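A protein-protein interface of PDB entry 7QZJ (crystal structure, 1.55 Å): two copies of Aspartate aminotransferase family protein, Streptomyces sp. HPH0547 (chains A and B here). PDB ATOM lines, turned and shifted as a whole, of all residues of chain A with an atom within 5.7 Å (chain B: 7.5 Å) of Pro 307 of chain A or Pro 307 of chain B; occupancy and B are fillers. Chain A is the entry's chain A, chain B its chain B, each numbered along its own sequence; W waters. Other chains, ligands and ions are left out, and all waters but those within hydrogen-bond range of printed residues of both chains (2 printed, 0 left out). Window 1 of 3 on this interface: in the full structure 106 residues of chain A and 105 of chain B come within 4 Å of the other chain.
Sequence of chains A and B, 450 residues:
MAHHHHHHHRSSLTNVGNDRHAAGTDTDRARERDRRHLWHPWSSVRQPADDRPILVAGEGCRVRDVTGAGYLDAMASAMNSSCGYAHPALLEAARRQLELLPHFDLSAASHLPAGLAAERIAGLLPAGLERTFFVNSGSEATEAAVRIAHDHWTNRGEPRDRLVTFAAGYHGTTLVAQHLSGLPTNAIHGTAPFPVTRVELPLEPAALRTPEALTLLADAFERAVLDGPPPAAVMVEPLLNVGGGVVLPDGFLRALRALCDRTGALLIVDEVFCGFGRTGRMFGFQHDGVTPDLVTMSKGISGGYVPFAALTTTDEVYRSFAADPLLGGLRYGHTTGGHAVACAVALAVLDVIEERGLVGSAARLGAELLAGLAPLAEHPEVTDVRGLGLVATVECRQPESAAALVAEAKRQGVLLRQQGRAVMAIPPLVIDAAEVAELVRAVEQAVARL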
ATOM      1  N   VAL A 135     -11.448  13.676  -4.063  1.00  0.00           N
ATOM      2  CA  VAL A 135     -10.363  13.902  -5.034  1.00  0.00           C
ATOM      3  C   VAL A 135      -9.900  12.549  -5.582  1.00  0.00           C
ATOM      4  O   VAL A 135     -10.531  11.521  -5.297  1.00  0.00           O
ATOM      5  CB  VAL A 135      -9.183  14.731  -4.467  1.00  0.00           C
ATOM      6  CG1 VAL A 135      -9.660  16.088  -3.966  1.00  0.00           C
ATOM      7  CG2 VAL A 135      -8.476  13.993  -3.353  1.00  0.00           C
ATOM      8  N   ASN A 136      -8.820  12.527  -6.373  1.00  0.00           N
ATOM      9  CA  ASN A 136      -8.390  11.289  -7.024  1.00  0.00           C
ATOM     10  C   ASN A 136      -7.311  10.549  -6.266  1.00  0.00           C
ATOM     11  O   ASN A 136      -7.280   9.340  -6.321  1.00  0.00           O
ATOM     12  CB  ASN A 136      -7.876  11.554  -8.437  1.00  0.00           C
ATOM     13  CG  ASN A 136      -8.881  12.290  -9.299  1.00  0.00           C
ATOM     14  OD1 ASN A 136      -9.931  11.748  -9.640  1.00  0.00           O
ATOM     15  ND2 ASN A 136      -8.581  13.521  -9.641  1.00  0.00           N
ATOM     16  N   SER A 302     -11.131   2.287  -2.071  1.00  0.00           N
ATOM     17  CA  SER A 302     -11.744   1.746  -3.292  1.00  0.00           C
ATOM     18  C   SER A 302     -11.152   0.393  -3.684  1.00  0.00           C
ATOM     19  O   SER A 302     -11.349  -0.073  -4.807  1.00  0.00           O
ATOM     20  CB  SER A 302     -11.575   2.753  -4.444  1.00  0.00           C
ATOM     21  OG  SER A 302     -10.202   2.884  -4.714  1.00  0.00           O
ATOM     22  N   GLY A 304      -8.259  -0.172  -4.517  1.00  0.00           N
ATOM     23  CA  GLY A 304      -7.430   0.067  -5.685  1.00  0.00           C
ATOM     24  C   GLY A 304      -8.123  -0.079  -7.027  1.00  0.00           C
ATOM     25  O   GLY A 304      -7.472   0.081  -8.075  1.00  0.00           O
ATOM     26  N   TYR A 305      -9.428  -0.338  -7.072  1.00  0.00           N
ATOM     27  CA  TYR A 305     -10.059  -0.677  -8.362  1.00  0.00           C
ATOM     28  C   TYR A 305     -10.372   0.540  -9.220  1.00  0.00           C
ATOM     29  O   TYR A 305     -10.472   0.423 -10.421  1.00  0.00           O
ATOM     30  CB  TYR A 305     -11.350  -1.458  -8.170  1.00  0.00           C
ATOM     31  CG  TYR A 305     -11.187  -2.931  -7.799  1.00  0.00           C
ATOM     32  CD1 TYR A 305     -10.092  -3.398  -7.073  1.00  0.00           C
ATOM     33  CD2 TYR A 305     -12.177  -3.836  -8.142  1.00  0.00           C
ATOM     34  CE1 TYR A 305      -9.989  -4.739  -6.709  1.00  0.00           C
ATOM     35  CE2 TYR A 305     -12.081  -5.167  -7.796  1.00  0.00           C
ATOM     36  CZ  TYR A 305     -10.986  -5.615  -7.080  1.00  0.00           C
ATOM     37  OH  TYR A 305     -10.892  -6.942  -6.691  1.00  0.00           O
ATOM     38  N   VAL A 306     -10.555   1.695  -8.585  1.00  0.00           N
ATOM     39  CA  VAL A 306     -10.683   2.995  -9.263  1.00  0.00           C
ATOM     40  C   VAL A 306      -9.904   4.013  -8.433  1.00  0.00           C
ATOM     41  O   VAL A 306     -10.064   4.046  -7.200  1.00  0.00           O
ATOM     42  CB  VAL A 306     -12.143   3.473  -9.296  1.00  0.00           C
ATOM     43  CG1 VAL A 306     -12.299   4.712 -10.161  1.00  0.00           C
ATOM     44  CG2 VAL A 306     -13.082   2.362  -9.787  1.00  0.00           C
ATOM     45  N   PRO A 307      -9.092   4.872  -9.071  1.00  0.00           N
ATOM     46  CA  PRO A 307      -8.458   5.953  -8.298  1.00  0.00           C
ATOM     47  C   PRO A 307      -9.474   6.765  -7.503  1.00  0.00           C
ATOM     48  O   PRO A 307     -10.464   7.199  -8.049  1.00  0.00           O
ATOM     49  CB  PRO A 307      -7.800   6.806  -9.372  1.00  0.00           C
ATOM     50  CG  PRO A 307      -7.504   5.827 -10.474  1.00  0.00           C
ATOM     51  CD  PRO A 307      -8.702   4.925 -10.489  1.00  0.00           C
ATOM     52  N   PHE A 308      -9.235   6.936  -6.205  1.00  0.00           N
ATOM     53  CA  PHE A 308     -10.198   7.588  -5.327  1.00  0.00           C
ATOM     54  C   PHE A 308      -9.513   8.037  -4.040  1.00  0.00           C
ATOM     55  O   PHE A 308      -8.615   7.359  -3.539  1.00  0.00           O
ATOM     56  CB  PHE A 308     -11.315   6.594  -4.965  1.00  0.00           C
ATOM     57  CG  PHE A 308     -12.548   7.206  -4.317  1.00  0.00           C
ATOM     58  CD1 PHE A 308     -13.222   8.259  -4.895  1.00  0.00           C
ATOM     59  CD2 PHE A 308     -13.086   6.637  -3.165  1.00  0.00           C
ATOM     60  CE1 PHE A 308     -14.358   8.803  -4.327  1.00  0.00           C
ATOM     61  CE2 PHE A 308     -14.232   7.167  -2.593  1.00  0.00           C
ATOM     62  CZ  PHE A 308     -14.876   8.238  -3.190  1.00  0.00           C
ATOM     63  N   ALA A 309      -9.930   9.199  -3.555  1.00  0.00           N
ATOM     64  CA  ALA A 309      -9.409   9.720  -2.306  1.00  0.00           C
ATOM     65  C   ALA A 309     -10.437  10.681  -1.731  1.00  0.00           C
ATOM     66  O   ALA A 309     -11.348  11.142  -2.419  1.00  0.00           O
ATOM     67  CB  ALA A 309      -8.065  10.383  -2.534  1.00  0.00           C
ATOM     68  N   THR A 336     -12.535  14.989 -12.207  1.00  0.00           N
ATOM     69  CA  THR A 336     -13.072  13.696 -11.783  1.00  0.00           C
ATOM     70  C   THR A 336     -13.136  13.514 -10.263  1.00  0.00           C
ATOM     71  O   THR A 336     -13.337  12.404  -9.805  1.00  0.00           O
ATOM     72  CB  THR A 336     -12.318  12.507 -12.437  1.00  0.00           C
ATOM     73  OG1 THR A 336     -10.939  12.501 -12.028  1.00  0.00           O
ATOM     74  CG2 THR A 336     -12.369  12.601 -13.936  1.00  0.00           C
ATOM     75  N   HIS A 339     -15.795  11.009  -8.614  1.00  0.00           N
ATOM     76  CA  HIS A 339     -16.126  10.061  -9.695  1.00  0.00           C
ATOM     77  C   HIS A 339     -17.165   9.032  -9.225  1.00  0.00           C
ATOM     78  O   HIS A 339     -16.961   8.374  -8.203  1.00  0.00           O
ATOM     79  CB  HIS A 339     -14.847   9.359 -10.136  1.00  0.00           C
ATOM     80  CG  HIS A 339     -14.956   8.669 -11.448  1.00  0.00           C
ATOM     81  ND1 HIS A 339     -15.304   7.339 -11.559  1.00  0.00           N
ATOM     82  CD2 HIS A 339     -14.804   9.128 -12.709  1.00  0.00           C
ATOM     83  CE1 HIS A 339     -15.309   7.001 -12.833  1.00  0.00           C
ATOM     84  NE2 HIS A 339     -15.014   8.068 -13.554  1.00  0.00           N
ATOM     85  N   ALA A 342     -16.000   5.376  -8.767  1.00  0.00           N
ATOM     86  CA  ALA A 342     -15.143   5.271  -7.589  1.00  0.00           C
ATOM     87  C   ALA A 342     -15.995   5.265  -6.320  1.00  0.00           C
ATOM     88  O   ALA A 342     -15.760   4.455  -5.438  1.00  0.00           O
ATOM     89  CB  ALA A 342     -14.137   6.407  -7.554  1.00  0.00           C
ATOM     90  N   ASN B  80     -15.377  15.880 -20.635  1.00  0.00           N
ATOM     91  CA  ASN B  80     -14.467  14.747 -20.872  1.00  0.00           C
ATOM     92  C   ASN B  80     -15.065  13.473 -21.454  1.00  0.00           C
ATOM     93  O   ASN B  80     -14.334  12.527 -21.733  1.00  0.00           O
ATOM     94  CB  ASN B  80     -13.722  14.411 -19.575  1.00  0.00           C
ATOM     95  CG  ASN B  80     -14.630  13.930 -18.470  1.00  0.00           C
ATOM     96  OD1 ASN B  80     -15.862  13.915 -18.603  1.00  0.00           O
ATOM     97  ND2 ASN B  80     -14.025  13.527 -17.370  1.00  0.00           N
ATOM     98  N   PRO B 102      -6.401  -4.796 -11.627  1.00  0.00           N
ATOM     99  CA  PRO B 102      -6.754  -3.358 -11.708  1.00  0.00           C
ATOM    100  C   PRO B 102      -5.550  -2.438 -11.866  1.00  0.00           C
ATOM    101  O   PRO B 102      -5.650  -1.403 -12.522  1.00  0.00           O
ATOM    102  CB  PRO B 102      -7.489  -3.096 -10.388  1.00  0.00           C
ATOM    103  CG  PRO B 102      -7.988  -4.475  -9.991  1.00  0.00           C
ATOM    104  CD  PRO B 102      -6.900  -5.406 -10.387  1.00  0.00           C
ATOM    105  N   VAL B 135      -0.428   9.742 -14.624  1.00  0.00           N
ATOM    106  CA  VAL B 135      -0.916  10.271 -13.350  1.00  0.00           C
ATOM    107  C   VAL B 135      -2.446  10.191 -13.377  1.00  0.00           C
ATOM    108  O   VAL B 135      -2.999   9.597 -14.309  1.00  0.00           O
ATOM    109  CB  VAL B 135      -0.381  11.701 -13.053  1.00  0.00           C
ATOM    110  CG1 VAL B 135       1.137  11.743 -12.983  1.00  0.00           C
ATOM    111  CG2 VAL B 135      -0.868  12.710 -14.075  1.00  0.00           C
ATOM    112  N   ASN B 136      -3.129  10.726 -12.357  1.00  0.00           N
ATOM    113  CA  ASN B 136      -4.595  10.583 -12.257  1.00  0.00           C
ATOM    114  C   ASN B 136      -5.386  11.755 -12.834  1.00  0.00           C
ATOM    115  O   ASN B 136      -6.467  11.542 -13.362  1.00  0.00           O
ATOM    116  CB  ASN B 136      -5.061  10.363 -10.817  1.00  0.00           C
ATOM    117  CG  ASN B 136      -4.351   9.223 -10.119  1.00  0.00           C
ATOM    118  OD1 ASN B 136      -4.576   8.049 -10.438  1.00  0.00           O
ATOM    119  ND2 ASN B 136      -3.479   9.554  -9.182  1.00  0.00           N
ATOM    120  N   SER B 137      -4.864  12.974 -12.731  1.00  0.00           N
ATOM    121  CA  SER B 137      -5.569  14.202 -13.092  1.00  0.00           C
ATOM    122  C   SER B 137      -4.711  15.154 -13.891  1.00  0.00           C
ATOM    123  O   SER B 137      -3.476  15.055 -13.903  1.00  0.00           O
ATOM    124  CB  SER B 137      -6.043  14.941 -11.848  1.00  0.00           C
ATOM    125  OG  SER B 137      -4.930  15.414 -11.084  1.00  0.00           O
ATOM    126  N   SER B 298      -5.473  14.689 -20.397  1.00  0.00           N
ATOM    127  CA  SER B 298      -6.405  14.057 -19.452  1.00  0.00           C
ATOM    128  C   SER B 298      -7.784  14.123 -20.143  1.00  0.00           C
ATOM    129  O   SER B 298      -7.840  14.011 -21.345  1.00  0.00           O
ATOM    130  CB  SER B 298      -6.409  14.772 -18.101  1.00  0.00           C
ATOM    131  OG  SER B 298      -7.152  14.045 -17.123  1.00  0.00           O
ATOM    132  N   ILE B 301      -9.158  11.456 -23.000  1.00  0.00           N
ATOM    133  CA  ILE B 301      -8.304  10.263 -23.095  1.00  0.00           C
ATOM    134  C   ILE B 301      -8.980   9.020 -22.525  1.00  0.00           C
ATOM    135  O   ILE B 301      -8.835   7.957 -23.085  1.00  0.00           O
ATOM    136  CB  ILE B 301      -6.915  10.535 -22.399  1.00  0.00           C
ATOM    137  CG1 ILE B 301      -5.892   9.454 -22.698  1.00  0.00           C
ATOM    138  CG2 ILE B 301      -7.048  10.674 -20.893  1.00  0.00           C
ATOM    139  CD1 ILE B 301      -4.517   9.805 -22.111  1.00  0.00           C
ATOM    140  N   SER B 302      -9.678   9.137 -21.397  1.00  0.00           N
ATOM    141  CA  SER B 302     -10.336   7.938 -20.845  1.00  0.00           C
ATOM    142  C   SER B 302     -11.845   8.032 -20.958  1.00  0.00           C
ATOM    143  O   SER B 302     -12.544   7.251 -20.327  1.00  0.00           O
ATOM    144  CB  SER B 302      -9.942   7.745 -19.383  1.00  0.00           C
ATOM    145  OG  SER B 302     -10.486   8.795 -18.616  1.00  0.00           O
ATOM    146  N   GLY B 304     -13.704   9.967 -19.589  1.00  0.00           N
ATOM    147  CA  GLY B 304     -14.227  10.180 -18.245  1.00  0.00           C
ATOM    148  C   GLY B 304     -14.560   8.912 -17.472  1.00  0.00           C
ATOM    149  O   GLY B 304     -15.024   9.007 -16.314  1.00  0.00           O
ATOM    150  N   TYR B 305     -14.346   7.736 -18.050  1.00  0.00           N
ATOM    151  CA  TYR B 305     -14.843   6.507 -17.410  1.00  0.00           C
ATOM    152  C   TYR B 305     -13.972   6.069 -16.240  1.00  0.00           C
ATOM    153  O   TYR B 305     -14.465   5.410 -15.337  1.00  0.00           O
ATOM    154  CB  TYR B 305     -14.978   5.359 -18.404  1.00  0.00           C
ATOM    155  CG  TYR B 305     -16.181   5.404 -19.324  1.00  0.00           C
ATOM    156  CD1 TYR B 305     -16.742   6.600 -19.756  1.00  0.00           C
ATOM    157  CD2 TYR B 305     -16.710   4.223 -19.824  1.00  0.00           C
ATOM    158  CE1 TYR B 305     -17.812   6.628 -20.624  1.00  0.00           C
ATOM    159  CE2 TYR B 305     -17.806   4.245 -20.695  1.00  0.00           C
ATOM    160  CZ  TYR B 305     -18.331   5.446 -21.094  1.00  0.00           C
ATOM    161  OH  TYR B 305     -19.386   5.496 -21.988  1.00  0.00           O
ATOM    162  N   VAL B 306     -12.680   6.426 -16.257  1.00  0.00           N
ATOM    163  CA  VAL B 306     -11.767   6.164 -15.147  1.00  0.00           C
ATOM    164  C   VAL B 306     -10.856   7.376 -15.053  1.00  0.00           C
ATOM    165  O   VAL B 306     -10.358   7.810 -16.074  1.00  0.00           O
ATOM    166  CB  VAL B 306     -10.871   4.937 -15.399  1.00  0.00           C
ATOM    167  CG1 VAL B 306     -10.051   4.585 -14.159  1.00  0.00           C
ATOM    168  CG2 VAL B 306     -11.706   3.732 -15.839  1.00  0.00           C
ATOM    169  N   PRO B 307     -10.613   7.910 -13.842  1.00  0.00           N
ATOM    170  CA  PRO B 307      -9.648   9.025 -13.734  1.00  0.00           C
ATOM    171  C   PRO B 307      -8.286   8.650 -14.350  1.00  0.00           C
ATOM    172  O   PRO B 307      -7.748   7.593 -14.044  1.00  0.00           O
ATOM    173  CB  PRO B 307      -9.543   9.236 -12.245  1.00  0.00           C
ATOM    174  CG  PRO B 307     -10.874   8.791 -11.731  1.00  0.00           C
ATOM    175  CD  PRO B 307     -11.212   7.591 -12.536  1.00  0.00           C
ATOM    176  N   PHE B 308      -7.781   9.489 -15.255  1.00  0.00           N
ATOM    177  CA  PHE B 308      -6.584   9.168 -16.008  1.00  0.00           C
ATOM    178  C   PHE B 308      -6.003  10.443 -16.567  1.00  0.00           C
ATOM    179  O   PHE B 308      -6.737  11.301 -17.002  1.00  0.00           O
ATOM    180  CB  PHE B 308      -6.922   8.241 -17.197  1.00  0.00           C
ATOM    181  CG  PHE B 308      -5.730   7.599 -17.861  1.00  0.00           C
ATOM    182  CD1 PHE B 308      -4.798   6.908 -17.110  1.00  0.00           C
ATOM    183  CD2 PHE B 308      -5.582   7.626 -19.220  1.00  0.00           C
ATOM    184  CE1 PHE B 308      -3.734   6.254 -17.703  1.00  0.00           C
ATOM    185  CE2 PHE B 308      -4.494   6.998 -19.822  1.00  0.00           C
ATOM    186  CZ  PHE B 308      -3.589   6.302 -19.060  1.00  0.00           C
ATOM    187  N   ALA B 309      -4.679  10.533 -16.557  1.00  0.00           N
ATOM    188  CA  ALA B 309      -3.971  11.645 -17.192  1.00  0.00           C
ATOM    189  C   ALA B 309      -2.577  11.198 -17.546  1.00  0.00           C
ATOM    190  O   ALA B 309      -2.113  10.160 -17.089  1.00  0.00           O
ATOM    191  CB  ALA B 309      -3.902  12.845 -16.253  1.00  0.00           C
ATOM    192  N   THR B 336      -1.696   5.220  -7.789  1.00  0.00           N
ATOM    193  CA  THR B 336      -2.502   4.688  -8.898  1.00  0.00           C
ATOM    194  C   THR B 336      -2.108   5.299 -10.242  1.00  0.00           C
ATOM    195  O   THR B 336      -2.844   5.140 -11.214  1.00  0.00           O
ATOM    196  CB  THR B 336      -4.007   4.820  -8.665  1.00  0.00           C
ATOM    197  OG1 THR B 336      -4.370   6.195  -8.520  1.00  0.00           O
ATOM    198  CG2 THR B 336      -4.451   4.099  -7.412  1.00  0.00           C
ATOM    199  N   GLY B 337      -0.951   5.967 -10.328  1.00  0.00           N
ATOM    200  CA  GLY B 337      -0.491   6.469 -11.620  1.00  0.00           C
ATOM    201  C   GLY B 337      -0.153   5.306 -12.536  1.00  0.00           C
ATOM    202  O   GLY B 337       0.670   4.459 -12.206  1.00  0.00           O
ATOM    203  N   GLY B 338      -0.786   5.271 -13.699  1.00  0.00           N
ATOM    204  CA  GLY B 338      -0.634   4.148 -14.635  1.00  0.00           C
ATOM    205  C   GLY B 338      -1.620   3.029 -14.369  1.00  0.00           C
ATOM    206  O   GLY B 338      -1.437   1.925 -14.869  1.00  0.00           O
ATOM    207  N   HIS B 339      -2.685   3.341 -13.642  1.00  0.00           N
ATOM    208  CA  HIS B 339      -3.780   2.394 -13.326  1.00  0.00           C
ATOM    209  C   HIS B 339      -4.141   1.553 -14.564  1.00  0.00           C
ATOM    210  O   HIS B 339      -4.429   2.109 -15.641  1.00  0.00           O
ATOM    211  CB  HIS B 339      -4.999   3.172 -12.831  1.00  0.00           C
ATOM    212  CG  HIS B 339      -6.019   2.325 -12.160  1.00  0.00           C
ATOM    213  ND1 HIS B 339      -7.133   1.846 -12.817  1.00  0.00           N
ATOM    214  CD2 HIS B 339      -6.124   1.894 -10.882  1.00  0.00           C
ATOM    215  CE1 HIS B 339      -7.865   1.145 -11.983  1.00  0.00           C
ATOM    216  NE2 HIS B 339      -7.268   1.145 -10.802  1.00  0.00           N
ATOM    217  N   VAL B 341      -6.716  -0.349 -15.434  1.00  0.00           N
ATOM    218  CA  VAL B 341      -8.067  -0.220 -15.983  1.00  0.00           C
ATOM    219  C   VAL B 341      -8.155   1.094 -16.775  1.00  0.00           C
ATOM    220  O   VAL B 341      -8.691   1.113 -17.882  1.00  0.00           O
ATOM    221  CB  VAL B 341      -9.174  -0.262 -14.930  1.00  0.00           C
ATOM    222  CG1 VAL B 341     -10.568  -0.258 -15.575  1.00  0.00           C
ATOM    223  CG2 VAL B 341      -9.010  -1.477 -14.032  1.00  0.00           C
ATOM    224  N   ALA B 342      -7.625   2.189 -16.208  1.00  0.00           N
ATOM    225  CA  ALA B 342      -7.577   3.468 -16.901  1.00  0.00           C
ATOM    226  C   ALA B 342      -6.856   3.312 -18.226  1.00  0.00           C
ATOM    227  O   ALA B 342      -7.348   3.807 -19.242  1.00  0.00           O
ATOM    228  CB  ALA B 342      -6.911   4.515 -16.048  1.00  0.00           C
ATOM    229  N   CYS B 343      -5.707   2.635 -18.233  1.00  0.00           N
ATOM    230  CA  CYS B 343      -4.941   2.430 -19.483  1.00  0.00           C
ATOM    231  C   CYS B 343      -5.762   1.618 -20.495  1.00  0.00           C
ATOM    232  O   CYS B 343      -5.805   1.950 -21.680  1.00  0.00           O
ATOM    233  CB  CYS B 343      -3.621   1.701 -19.232  1.00  0.00           C
ATOM    234  SG  CYS B 343      -2.371   2.695 -18.340  1.00  0.00           S
HETATM  235  O   HOH W   1      -5.631   7.181  -6.246  1.00  0.00           O
HETATM  236  O   HOH W   2      -8.835  12.626 -13.842  1.00  0.00           O
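Of the printed residues of chain B, Pro 307 of chain A touches Asn 136 (3.6 Å), Val 306 (3.9 Å), Pro 307 (3.99 Å), Thr 336 (3.6 Å) and His 339 (3.998 Å). Of the printed residues of chain B, Tyr 305 of chain A touches Pro 102 (3.8 Å) and His 339 (3.1 Å). Printed residues of chain B within 4 Å of Asn 136 of chain A: Asn 136 (3.9 Å), Ser 137 (3.7 Å) and Pro 307 (3.6 Å). Printed residues of chain A within 4 Å of Asn 80 of chain B: Thr 336 (3.9 Å). Of the printed residues of chain A, Ser 137 of chain B touches Asn 136. Printed residues of chain B within 4 Å of Thr 336 of chain A: Asn 80 (3.9 Å) and Pro 307 (3.6 Å). Val 135 of chain B touches none of the printed residues of chain A. Ala 342 of chain A touches none of the printed residues of chain B. The nearest printed residue of chain A that does not touch Pro 307 of chain B is Ala 342 of chain A (5.8 Å).
O of Tyr 305 of chain B lies close to NE2 of His 339 of chain A (3.2 Å). NE2 of His 339 of chain A is in hydrogen-bond range of O of Gly 304 of chain B, at 2.9 Å. O of Gly 304 of chain A sits at hydrogen-bond distance from NE2 of His 339 of chain B, 2.9 Å away. The backbone carbonyl oxygen (O) of Tyr 305 of chain A lies close to a ring nitrogen (NE2) of His 339 of chain B, at 3.3 Å.
The backbone NH (N) of Ala 342 of chain A sits at hydrogen-bond distance from a ring nitrogen (ND1) of His 339 of chain A (3.5 Å). O of Val 306 of chain B is in hydrogen-bond range of OG of Ser 302 of chain B (2.7 Å). The backbone carbonyl oxygen (O) of Val 306 of chain A lies within hydrogen-bond range of the side-chain hydroxyl (OG) of Ser 302 of chain A, 2.7 Å away. The side-chain amide oxygen of Asn 136 of chain A is in hydrogen-bond range of the side-chain hydroxyl of Thr 336 of chain A (2.7 Å). O of Asn 80 of chain B is in hydrogen-bond range of N of Gly 304 of chain B (3.4 Å). The backbone carbonyl oxygen (O) of Pro 102 of chain B sits at hydrogen-bond distance from the backbone NH (N) of Val 341 of chain B, 3.3 Å away.
Water W2 lies within hydrogen-bond range of O of Asn 136 of chain B (2.6 Å) and OG1 of Thr 336 of chain A (2.8 Å). Water W1 lies within hydrogen-bond range of O of Asn 136 of chain A (2.7 Å) and OG1 of Thr 336 of chain B (2.8 Å).
Of the 12 printed residues of chain A, 7 touch a printed residue of chain B. Printed residues of chain A that touch a printed residue of chain B: Asn 136, Gly 304, Tyr 305, Val 306, Pro 307, Thr 336 and His 339. Of the 21 printed residues of chain B, 10 touch a printed residue of chain A. Hydrophobic or aromatic side chains of chain B within 4 Å of the printed part of chain A: Pro 102, Val 306, Pro 307 and His 339. Among the printed residues, 19 pairs touch across the chains.
ND2 of Asn 136 of chain A touches CB of Ser 137 of chain B (3.7 Å). Gly 304 of chain A touches Pro 102 of chain B. CD1 of Tyr 305 of chain A touches CG of Pro 102 of chain B, 3.8 Å away. Pro 307 of chain B touches Val 306 of chain A (CD to CG1, 3.9 Å). CD of Pro 307 of chain A touches CG1 of Val 306 of chain B, 3.9 Å away. Thr 336 of chain B touches Pro 307 of chain A. CD of Pro 307 of chain A touches CD2 of His 339 of chain B (3.998 Å). Pro 307 of chain B touches Thr 336 of chain A. Val 306 of chain B touches His 339 of chain A (N to NE2, 3.9 Å). CD2 of His 339 of chain A touches CD of Pro 307 of chain B, 3.9 Å away.
Asn 136 of chain B touches its own counterpart, Asn 136 of chain A. Tyr 305 of chain A touches His 339 of chain B, and with the chains exchanged His 339 of chain A touches Tyr 305 of chain B. Val 306 of chain A touches Pro 307 of chain B, and with the chains exchanged Pro 307 of chain A touches Val 306 of chain B. Pro 307 of chain A touches Thr 336 of chain B, and with the chains exchanged Thr 336 of chain A touches Pro 307 of chain B. Positions printed for both chains: 135, 136, 302, 304, 305, 306, 307, 308, 309, 336, 339 and 342. Of the 19 pairs that touch across the chains among the printed residues, 14 have their exchanged pair printed and touching as well.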
